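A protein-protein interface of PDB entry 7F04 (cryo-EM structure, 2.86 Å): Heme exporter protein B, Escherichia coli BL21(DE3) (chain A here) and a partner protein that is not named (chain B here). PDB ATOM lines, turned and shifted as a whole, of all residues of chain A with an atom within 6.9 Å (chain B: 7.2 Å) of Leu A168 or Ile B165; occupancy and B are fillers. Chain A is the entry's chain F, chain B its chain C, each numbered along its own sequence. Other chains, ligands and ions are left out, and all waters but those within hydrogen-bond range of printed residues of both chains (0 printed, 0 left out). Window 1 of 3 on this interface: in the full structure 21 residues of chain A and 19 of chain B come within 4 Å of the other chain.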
ATOM      1  N   LEU A 143       2.980  12.378  28.419  1.00  0.00           N
ATOM      2  CA  LEU A 143       2.354  13.694  28.459  1.00  0.00           C
ATOM      3  C   LEU A 143       2.585  14.454  27.161  1.00  0.00           C
ATOM      4  O   LEU A 143       1.713  15.208  26.713  1.00  0.00           O
ATOM      5  CB  LEU A 143       2.888  14.494  29.645  1.00  0.00           C
ATOM      6  CG  LEU A 143       2.358  14.128  31.030  1.00  0.00           C
ATOM      7  CD1 LEU A 143       3.229  14.750  32.104  1.00  0.00           C
ATOM      8  CD2 LEU A 143       0.915  14.569  31.186  1.00  0.00           C
ATOM      9  N   GLY A 144       3.756  14.279  26.545  1.00  0.00           N
ATOM     10  CA  GLY A 144       4.044  14.979  25.308  1.00  0.00           C
ATOM     11  C   GLY A 144       3.450  14.351  24.069  1.00  0.00           C
ATOM     12  O   GLY A 144       3.374  15.016  23.032  1.00  0.00           O
ATOM     13  N   PRO A 146       0.180  13.455  23.382  1.00  0.00           N
ATOM     14  CA  PRO A 146      -1.014  14.154  22.874  1.00  0.00           C
ATOM     15  C   PRO A 146      -0.708  15.498  22.236  1.00  0.00           C
ATOM     16  O   PRO A 146      -1.349  15.864  21.245  1.00  0.00           O
ATOM     17  CB  PRO A 146      -1.887  14.303  24.125  1.00  0.00           C
ATOM     18  CG  PRO A 146      -1.432  13.237  25.032  1.00  0.00           C
ATOM     19  CD  PRO A 146       0.038  13.144  24.813  1.00  0.00           C
ATOM     20  N   GLY A 147       0.257  16.245  22.772  1.00  0.00           N
ATOM     21  CA  GLY A 147       0.581  17.536  22.189  1.00  0.00           C
ATOM     22  C   GLY A 147       1.176  17.421  20.799  1.00  0.00           C
ATOM     23  O   GLY A 147       0.790  18.155  19.885  1.00  0.00           O
ATOM     24  N   LEU A 150      -1.535  16.490  18.429  1.00  0.00           N
ATOM     25  CA  LEU A 150      -2.377  17.616  18.044  1.00  0.00           C
ATOM     26  C   LEU A 150      -1.658  18.539  17.069  1.00  0.00           C
ATOM     27  O   LEU A 150      -2.281  19.092  16.156  1.00  0.00           O
ATOM     28  CB  LEU A 150      -2.816  18.393  19.284  1.00  0.00           C
ATOM     29  CG  LEU A 150      -3.827  17.724  20.215  1.00  0.00           C
ATOM     30  CD1 LEU A 150      -3.855  18.428  21.559  1.00  0.00           C
ATOM     31  CD2 LEU A 150      -5.205  17.714  19.589  1.00  0.00           C
ATOM     32  N   ILE A 163       4.345  24.955  24.617  1.00  0.00           N
ATOM     33  CA  ILE A 163       3.366  25.653  25.440  1.00  0.00           C
ATOM     34  C   ILE A 163       2.112  24.830  25.665  1.00  0.00           C
ATOM     35  O   ILE A 163       1.237  25.251  26.433  1.00  0.00           O
ATOM     36  CB  ILE A 163       3.003  27.030  24.849  1.00  0.00           C
ATOM     37  CG1 ILE A 163       2.054  26.880  23.664  1.00  0.00           C
ATOM     38  CG2 ILE A 163       4.252  27.784  24.432  1.00  0.00           C
ATOM     39  CD1 ILE A 163       1.500  28.193  23.171  1.00  0.00           C
ATOM     40  N   LEU A 164       1.995  23.670  25.024  1.00  0.00           N
ATOM     41  CA  LEU A 164       0.892  22.745  25.248  1.00  0.00           C
ATOM     42  C   LEU A 164       1.224  21.668  26.273  1.00  0.00           C
ATOM     43  O   LEU A 164       0.420  21.397  27.168  1.00  0.00           O
ATOM     44  CB  LEU A 164       0.468  22.087  23.929  1.00  0.00           C
ATOM     45  CG  LEU A 164      -0.529  22.806  23.018  1.00  0.00           C
ATOM     46  CD1 LEU A 164       0.055  24.037  22.379  1.00  0.00           C
ATOM     47  CD2 LEU A 164      -1.010  21.843  21.948  1.00  0.00           C
ATOM     48  N   VAL A 165       2.399  21.046  26.164  1.00  0.00           N
ATOM     49  CA  VAL A 165       2.750  19.931  27.037  1.00  0.00           C
ATOM     50  C   VAL A 165       3.730  20.315  28.133  1.00  0.00           C
ATOM     51  O   VAL A 165       4.060  19.464  28.973  1.00  0.00           O
ATOM     52  CB  VAL A 165       3.321  18.747  26.230  1.00  0.00           C
ATOM     53  CG1 VAL A 165       2.284  18.227  25.256  1.00  0.00           C
ATOM     54  CG2 VAL A 165       4.569  19.167  25.499  1.00  0.00           C
ATOM     55  N   LEU A 166       4.210  21.550  28.152  1.00  0.00           N
ATOM     56  CA  LEU A 166       5.141  21.974  29.189  1.00  0.00           C
ATOM     57  C   LEU A 166       4.414  22.330  30.484  1.00  0.00           C
ATOM     58  O   LEU A 166       4.914  22.000  31.566  1.00  0.00           O
ATOM     59  CB  LEU A 166       5.994  23.144  28.697  1.00  0.00           C
ATOM     60  CG  LEU A 166       7.365  23.311  29.346  1.00  0.00           C
ATOM     61  CD1 LEU A 166       8.144  22.017  29.264  1.00  0.00           C
ATOM     62  CD2 LEU A 166       8.138  24.424  28.665  1.00  0.00           C
ATOM     63  N   PRO A 167       3.261  23.013  30.443  1.00  0.00           N
ATOM     64  CA  PRO A 167       2.485  23.168  31.684  1.00  0.00           C
ATOM     65  C   PRO A 167       2.031  21.852  32.287  1.00  0.00           C
ATOM     66  O   PRO A 167       1.859  21.770  33.508  1.00  0.00           O
ATOM     67  CB  PRO A 167       1.293  24.026  31.244  1.00  0.00           C
ATOM     68  CG  PRO A 167       1.798  24.793  30.100  1.00  0.00           C
ATOM     69  CD  PRO A 167       2.713  23.863  29.370  1.00  0.00           C
ATOM     70  N   LEU A 168       1.824  20.819  31.470  1.00  0.00           N
ATOM     71  CA  LEU A 168       1.330  19.547  31.983  1.00  0.00           C
ATOM     72  C   LEU A 168       2.385  18.778  32.764  1.00  0.00           C
ATOM     73  O   LEU A 168       2.031  17.890  33.545  1.00  0.00           O
ATOM     74  CB  LEU A 168       0.807  18.687  30.834  1.00  0.00           C
ATOM     75  CG  LEU A 168      -0.189  19.359  29.891  1.00  0.00           C
ATOM     76  CD1 LEU A 168      -0.507  18.447  28.725  1.00  0.00           C
ATOM     77  CD2 LEU A 168      -1.454  19.740  30.636  1.00  0.00           C
ATOM     78  N   THR A 169       3.661  19.094  32.575  1.00  0.00           N
ATOM     79  CA  THR A 169       4.748  18.409  33.261  1.00  0.00           C
ATOM     80  C   THR A 169       5.126  19.067  34.579  1.00  0.00           C
ATOM     81  O   THR A 169       6.101  18.646  35.206  1.00  0.00           O
ATOM     82  CB  THR A 169       5.981  18.339  32.358  1.00  0.00           C
ATOM     83  OG1 THR A 169       6.432  19.665  32.064  1.00  0.00           O
ATOM     84  CG2 THR A 169       5.648  17.628  31.061  1.00  0.00           C
ATOM     85  N   ILE A 170       4.388  20.093  35.000  1.00  0.00           N
ATOM     86  CA  ILE A 170       4.730  20.795  36.238  1.00  0.00           C
ATOM     87  C   ILE A 170       4.614  19.903  37.469  1.00  0.00           C
ATOM     88  O   ILE A 170       5.531  19.925  38.304  1.00  0.00           O
ATOM     89  CB  ILE A 170       3.905  22.089  36.352  1.00  0.00           C
ATOM     90  CG1 ILE A 170       4.507  23.165  35.453  1.00  0.00           C
ATOM     91  CG2 ILE A 170       3.854  22.574  37.788  1.00  0.00           C
ATOM     92  CD1 ILE A 170       3.552  24.259  35.090  1.00  0.00           C
ATOM     93  N   PRO A 171       3.533  19.133  37.670  1.00  0.00           N
ATOM     94  CA  PRO A 171       3.513  18.232  38.836  1.00  0.00           C
ATOM     95  C   PRO A 171       4.640  17.214  38.836  1.00  0.00           C
ATOM     96  O   PRO A 171       5.215  16.924  39.894  1.00  0.00           O
ATOM     97  CB  PRO A 171       2.136  17.560  38.734  1.00  0.00           C
ATOM     98  CG  PRO A 171       1.704  17.760  37.335  1.00  0.00           C
ATOM     99  CD  PRO A 171       2.258  19.080  36.936  1.00  0.00           C
ATOM    100  N   LEU A 172       4.977  16.669  37.666  1.00  0.00           N
ATOM    101  CA  LEU A 172       6.082  15.721  37.582  1.00  0.00           C
ATOM    102  C   LEU A 172       7.396  16.387  37.961  1.00  0.00           C
ATOM    103  O   LEU A 172       8.186  15.829  38.727  1.00  0.00           O
ATOM    104  CB  LEU A 172       6.160  15.132  36.175  1.00  0.00           C
ATOM    105  CG  LEU A 172       7.489  14.483  35.793  1.00  0.00           C
ATOM    106  CD1 LEU A 172       7.699  13.202  36.578  1.00  0.00           C
ATOM    107  CD2 LEU A 172       7.533  14.212  34.305  1.00  0.00           C
ATOM    108  N   LEU A 173       7.634  17.593  37.442  1.00  0.00           N
ATOM    109  CA  LEU A 173       8.832  18.342  37.808  1.00  0.00           C
ATOM    110  C   LEU A 173       8.884  18.597  39.305  1.00  0.00           C
ATOM    111  O   LEU A 173       9.923  18.391  39.943  1.00  0.00           O
ATOM    112  CB  LEU A 173       8.863  19.667  37.047  1.00  0.00           C
ATOM    113  CG  LEU A 173      10.063  20.594  37.251  1.00  0.00           C
ATOM    114  CD1 LEU A 173      11.347  19.947  36.778  1.00  0.00           C
ATOM    115  CD2 LEU A 173       9.833  21.916  36.546  1.00  0.00           C
ATOM    116  N   ALA A 210      -5.980   9.519  24.424  1.00  0.00           N
ATOM    117  CA  ALA A 210      -5.995  10.922  24.026  1.00  0.00           C
ATOM    118  C   ALA A 210      -5.183  11.139  22.758  1.00  0.00           C
ATOM    119  O   ALA A 210      -5.595  11.890  21.866  1.00  0.00           O
ATOM    120  CB  ALA A 210      -5.464  11.795  25.161  1.00  0.00           C
ATOM    121  N   THR A 211      -4.028  10.480  22.655  1.00  0.00           N
ATOM    122  CA  THR A 211      -3.190  10.603  21.470  1.00  0.00           C
ATOM    123  C   THR A 211      -3.861   9.988  20.252  1.00  0.00           C
ATOM    124  O   THR A 211      -3.751  10.522  19.146  1.00  0.00           O
ATOM    125  CB  THR A 211      -1.835   9.947  21.723  1.00  0.00           C
ATOM    126  OG1 THR A 211      -1.266  10.476  22.924  1.00  0.00           O
ATOM    127  CG2 THR A 211      -0.891  10.212  20.569  1.00  0.00           C
ATOM    128  N   ALA A 214      -6.432  12.480  19.136  1.00  0.00           N
ATOM    129  CA  ALA A 214      -5.787  13.623  18.498  1.00  0.00           C
ATOM    130  C   ALA A 214      -5.270  13.268  17.109  1.00  0.00           C
ATOM    131  O   ALA A 214      -5.345  14.082  16.182  1.00  0.00           O
ATOM    132  CB  ALA A 214      -4.654  14.139  19.379  1.00  0.00           C
ATOM    133  N   TYR B  71     -12.878  28.203  32.582  1.00  0.00           N
ATOM    134  CA  TYR B  71     -12.192  26.977  32.175  1.00  0.00           C
ATOM    135  C   TYR B  71     -13.064  25.748  32.403  1.00  0.00           C
ATOM    136  O   TYR B  71     -13.056  24.817  31.591  1.00  0.00           O
ATOM    137  CB  TYR B  71     -10.857  26.825  32.896  1.00  0.00           C
ATOM    138  CG  TYR B  71      -9.903  25.936  32.133  1.00  0.00           C
ATOM    139  CD1 TYR B  71      -9.224  26.409  31.021  1.00  0.00           C
ATOM    140  CD2 TYR B  71      -9.708  24.614  32.503  1.00  0.00           C
ATOM    141  CE1 TYR B  71      -8.365  25.599  30.312  1.00  0.00           C
ATOM    142  CE2 TYR B  71      -8.851  23.796  31.799  1.00  0.00           C
ATOM    143  CZ  TYR B  71      -8.182  24.293  30.705  1.00  0.00           C
ATOM    144  OH  TYR B  71      -7.325  23.482  30.002  1.00  0.00           O
ATOM    145  N   LEU B 138      -2.381  27.332  30.296  1.00  0.00           N
ATOM    146  CA  LEU B 138      -3.356  26.466  29.639  1.00  0.00           C
ATOM    147  C   LEU B 138      -4.252  27.260  28.695  1.00  0.00           C
ATOM    148  O   LEU B 138      -4.539  26.820  27.574  1.00  0.00           O
ATOM    149  CB  LEU B 138      -4.200  25.738  30.683  1.00  0.00           C
ATOM    150  CG  LEU B 138      -3.484  24.811  31.663  1.00  0.00           C
ATOM    151  CD1 LEU B 138      -4.489  24.177  32.605  1.00  0.00           C
ATOM    152  CD2 LEU B 138      -2.694  23.746  30.929  1.00  0.00           C
ATOM    153  N   ALA B 158      -9.382  19.741  17.992  1.00  0.00           N
ATOM    154  CA  ALA B 158      -8.074  19.779  18.632  1.00  0.00           C
ATOM    155  C   ALA B 158      -8.099  20.652  19.878  1.00  0.00           C
ATOM    156  O   ALA B 158      -7.533  20.286  20.915  1.00  0.00           O
ATOM    157  CB  ALA B 158      -7.023  20.281  17.645  1.00  0.00           C
ATOM    158  N   ALA B 159      -8.755  21.811  19.796  1.00  0.00           N
ATOM    159  CA  ALA B 159      -8.873  22.680  20.961  1.00  0.00           C
ATOM    160  C   ALA B 159      -9.684  22.012  22.063  1.00  0.00           C
ATOM    161  O   ALA B 159      -9.350  22.131  23.246  1.00  0.00           O
ATOM    162  CB  ALA B 159      -9.502  24.013  20.560  1.00  0.00           C
ATOM    163  N   GLY B 160     -10.750  21.301  21.696  1.00  0.00           N
ATOM    164  CA  GLY B 160     -11.530  20.590  22.696  1.00  0.00           C
ATOM    165  C   GLY B 160     -10.749  19.478  23.368  1.00  0.00           C
ATOM    166  O   GLY B 160     -10.843  19.284  24.582  1.00  0.00           O
ATOM    167  N   ILE B 161      -9.966  18.730  22.587  1.00  0.00           N
ATOM    168  CA  ILE B 161      -9.142  17.671  23.164  1.00  0.00           C
ATOM    169  C   ILE B 161      -8.083  18.262  24.086  1.00  0.00           C
ATOM    170  O   ILE B 161      -7.812  17.724  25.167  1.00  0.00           O
ATOM    171  CB  ILE B 161      -8.518  16.814  22.047  1.00  0.00           C
ATOM    172  CG1 ILE B 161      -9.562  15.855  21.478  1.00  0.00           C
ATOM    173  CG2 ILE B 161      -7.330  16.028  22.565  1.00  0.00           C
ATOM    174  CD1 ILE B 161      -9.033  14.967  20.395  1.00  0.00           C
ATOM    175  N   LEU B 162      -7.475  19.378  23.681  1.00  0.00           N
ATOM    176  CA  LEU B 162      -6.500  20.040  24.541  1.00  0.00           C
ATOM    177  C   LEU B 162      -7.144  20.529  25.830  1.00  0.00           C
ATOM    178  O   LEU B 162      -6.543  20.438  26.906  1.00  0.00           O
ATOM    179  CB  LEU B 162      -5.846  21.202  23.799  1.00  0.00           C
ATOM    180  CG  LEU B 162      -4.712  21.900  24.549  1.00  0.00           C
ATOM    181  CD1 LEU B 162      -3.555  20.943  24.772  1.00  0.00           C
ATOM    182  CD2 LEU B 162      -4.251  23.128  23.800  1.00  0.00           C
ATOM    183  N   VAL B 163      -8.364  21.062  25.743  1.00  0.00           N
ATOM    184  CA  VAL B 163      -9.058  21.529  26.937  1.00  0.00           C
ATOM    185  C   VAL B 163      -9.353  20.365  27.872  1.00  0.00           C
ATOM    186  O   VAL B 163      -9.213  20.484  29.094  1.00  0.00           O
ATOM    187  CB  VAL B 163     -10.343  22.283  26.548  1.00  0.00           C
ATOM    188  CG1 VAL B 163     -11.261  22.415  27.740  1.00  0.00           C
ATOM    189  CG2 VAL B 163     -10.002  23.649  26.003  1.00  0.00           C
ATOM    190  N   LEU B 164      -9.774  19.228  27.317  1.00  0.00           N
ATOM    191  CA  LEU B 164     -10.036  18.055  28.148  1.00  0.00           C
ATOM    192  C   LEU B 164      -8.762  17.557  28.820  1.00  0.00           C
ATOM    193  O   LEU B 164      -8.770  17.203  30.008  1.00  0.00           O
ATOM    194  CB  LEU B 164     -10.669  16.952  27.305  1.00  0.00           C
ATOM    195  CG  LEU B 164     -12.143  17.161  26.968  1.00  0.00           C
ATOM    196  CD1 LEU B 164     -12.683  15.976  26.200  1.00  0.00           C
ATOM    197  CD2 LEU B 164     -12.948  17.393  28.233  1.00  0.00           C
ATOM    198  N   ILE B 165      -7.654  17.530  28.076  1.00  0.00           N
ATOM    199  CA  ILE B 165      -6.374  17.128  28.652  1.00  0.00           C
ATOM    200  C   ILE B 165      -5.983  18.066  29.784  1.00  0.00           C
ATOM    201  O   ILE B 165      -5.542  17.627  30.852  1.00  0.00           O
ATOM    202  CB  ILE B 165      -5.290  17.084  27.558  1.00  0.00           C
ATOM    203  CG1 ILE B 165      -5.532  15.912  26.610  1.00  0.00           C
ATOM    204  CG2 ILE B 165      -3.910  16.986  28.174  1.00  0.00           C
ATOM    205  CD1 ILE B 165      -4.826  16.055  25.289  1.00  0.00           C
ATOM    206  N   GLY B 166      -6.142  19.373  29.572  1.00  0.00           N
ATOM    207  CA  GLY B 166      -5.775  20.332  30.599  1.00  0.00           C
ATOM    208  C   GLY B 166      -6.653  20.251  31.832  1.00  0.00           C
ATOM    209  O   GLY B 166      -6.168  20.390  32.957  1.00  0.00           O
ATOM    210  N   VAL B 167      -7.956  20.037  31.643  1.00  0.00           N
ATOM    211  CA  VAL B 167      -8.856  19.993  32.790  1.00  0.00           C
ATOM    212  C   VAL B 167      -8.672  18.701  33.573  1.00  0.00           C
ATOM    213  O   VAL B 167      -8.898  18.675  34.788  1.00  0.00           O
ATOM    214  CB  VAL B 167     -10.318  20.186  32.352  1.00  0.00           C
ATOM    215  CG1 VAL B 167     -10.830  18.974  31.605  1.00  0.00           C
ATOM    216  CG2 VAL B 167     -11.196  20.493  33.553  1.00  0.00           C
ATOM    217  N   VAL B 168      -8.271  17.614  32.912  1.00  0.00           N
ATOM    218  CA  VAL B 168      -7.922  16.407  33.658  1.00  0.00           C
ATOM    219  C   VAL B 168      -6.694  16.659  34.523  1.00  0.00           C
ATOM    220  O   VAL B 168      -6.651  16.268  35.695  1.00  0.00           O
ATOM    221  CB  VAL B 168      -7.712  15.226  32.696  1.00  0.00           C
ATOM    222  CG1 VAL B 168      -6.936  14.114  33.379  1.00  0.00           C
ATOM    223  CG2 VAL B 168      -9.050  14.712  32.195  1.00  0.00           C
ATOM    224  N   ASN B 169      -5.687  17.331  33.969  1.00  0.00           N
ATOM    225  CA  ASN B 169      -4.444  17.596  34.678  1.00  0.00           C
ATOM    226  C   ASN B 169      -4.521  18.804  35.600  1.00  0.00           C
ATOM    227  O   ASN B 169      -3.606  19.000  36.404  1.00  0.00           O
ATOM    228  CB  ASN B 169      -3.305  17.802  33.676  1.00  0.00           C
ATOM    229  CG  ASN B 169      -2.767  16.499  33.127  1.00  0.00           C
ATOM    230  OD1 ASN B 169      -1.831  15.921  33.676  1.00  0.00           O
ATOM    231  ND2 ASN B 169      -3.356  16.030  32.036  1.00  0.00           N
ATOM    232  N   LEU B 170      -5.574  19.614  35.505  1.00  0.00           N
ATOM    233  CA  LEU B 170      -5.644  20.836  36.304  1.00  0.00           C
ATOM    234  C   LEU B 170      -5.663  20.576  37.807  1.00  0.00           C
ATOM    235  O   LEU B 170      -4.895  21.233  38.527  1.00  0.00           O
ATOM    236  CB  LEU B 170      -6.850  21.672  35.862  1.00  0.00           C
ATOM    237  CG  LEU B 170      -6.930  23.099  36.402  1.00  0.00           C
ATOM    238  CD1 LEU B 170      -5.585  23.797  36.286  1.00  0.00           C
ATOM    239  CD2 LEU B 170      -8.003  23.886  35.673  1.00  0.00           C
ATOM    240  N   ILE B 172      -4.416  18.064  39.392  1.00  0.00           N
ATOM    241  CA  ILE B 172      -3.089  17.555  39.723  1.00  0.00           C
ATOM    242  C   ILE B 172      -2.098  18.705  39.842  1.00  0.00           C
ATOM    243  O   ILE B 172      -1.334  18.793  40.809  1.00  0.00           O
ATOM    244  CB  ILE B 172      -2.633  16.528  38.672  1.00  0.00           C
ATOM    245  CG1 ILE B 172      -3.646  15.393  38.558  1.00  0.00           C
ATOM    246  CG2 ILE B 172      -1.264  15.977  39.020  1.00  0.00           C
ATOM    247  CD1 ILE B 172      -3.499  14.582  37.296  1.00  0.00           C
ATOM    248  N   ILE B 173      -2.111  19.612  38.863  1.00  0.00           N
ATOM    249  CA  ILE B 173      -1.200  20.751  38.887  1.00  0.00           C
ATOM    250  C   ILE B 173      -1.490  21.640  40.086  1.00  0.00           C
ATOM    251  O   ILE B 173      -0.570  22.106  40.767  1.00  0.00           O
ATOM    252  CB  ILE B 173      -1.288  21.542  37.569  1.00  0.00           C
ATOM    253  CG1 ILE B 173      -0.909  20.659  36.382  1.00  0.00           C
ATOM    254  CG2 ILE B 173      -0.382  22.752  37.619  1.00  0.00           C
ATOM    255  CD1 ILE B 173      -1.168  21.300  35.042  1.00  0.00           C
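Hydrophobic or aromatic side chains of chain B within 4 Å of the printed part of chain A: Ala B158, Ile B161, Leu B162, Ile B165, Ile B172 and Ile B173. Along chain B the printed residues that touch a printed residue of chain A span positions 158 to 173. Of the 19 printed residues of chain A, 8 touch a printed residue of chain B. Printed residues of chain A that touch a printed residue of chain B: Leu A143, Pro A146, Leu A150, Leu A164, Pro A167, Leu A168, Pro A171 and Ala A214. Hydrophobic or aromatic side chains of chain A within 4 Å of the printed part of chain B: Leu A143, Pro A146, Leu A150, Leu A164, Leu A168 and Pro A171. Along chain A the printed residues that touch a printed residue of chain B span positions 143 to 214. Among the printed residues, 9 pairs touch across the chains.
O of Ile B165 is in hydrogen-bond range of ND2 of Asn B169, 3.0 Å away.
Leu A168 touches one residue of chain B. Of the printed residues of chain A, Ile B165 touches Pro A146 (3.6 Å) and Leu A168 (3.7 Å). Of the printed residues of chain B, Pro A167 touches Ile B173. Of the printed residues of chain A, Ile B161 touches Ala A214. Of the printed residues of chain B, Pro A146 touches Ile B165 (3.6 Å). Printed residues of chain A within 4 Å of Ala B158: Leu A150. Leu A173 touches none of the printed residues of chain B. Val B168 touches none of the printed residues of chain A. The nearest residue of chain B that does not touch Leu A168 is Asn B169 (4.1 Å). The nearest residue of chain A that does not touch Ile B165 is Ala A210 (4.3 Å).
Among the printed residues, merely in contact across the chains: Pro A167 with Ile B173 (3.4 Å), Pro A171 with Ile B173 (3.6 Å), Pro A146 with Ile B165 (3.6 Å), Leu A150 with Ala B158 (3.7 Å), Leu A168 with Ile B165 (3.7 Å), Pro A171 with Ile B172 (3.8 Å), Ala A214 with Ile B161 (3.8 Å), Leu A164 with Leu B162 (3.8 Å) and Leu A143 with Asn B169 (3.9 Å).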
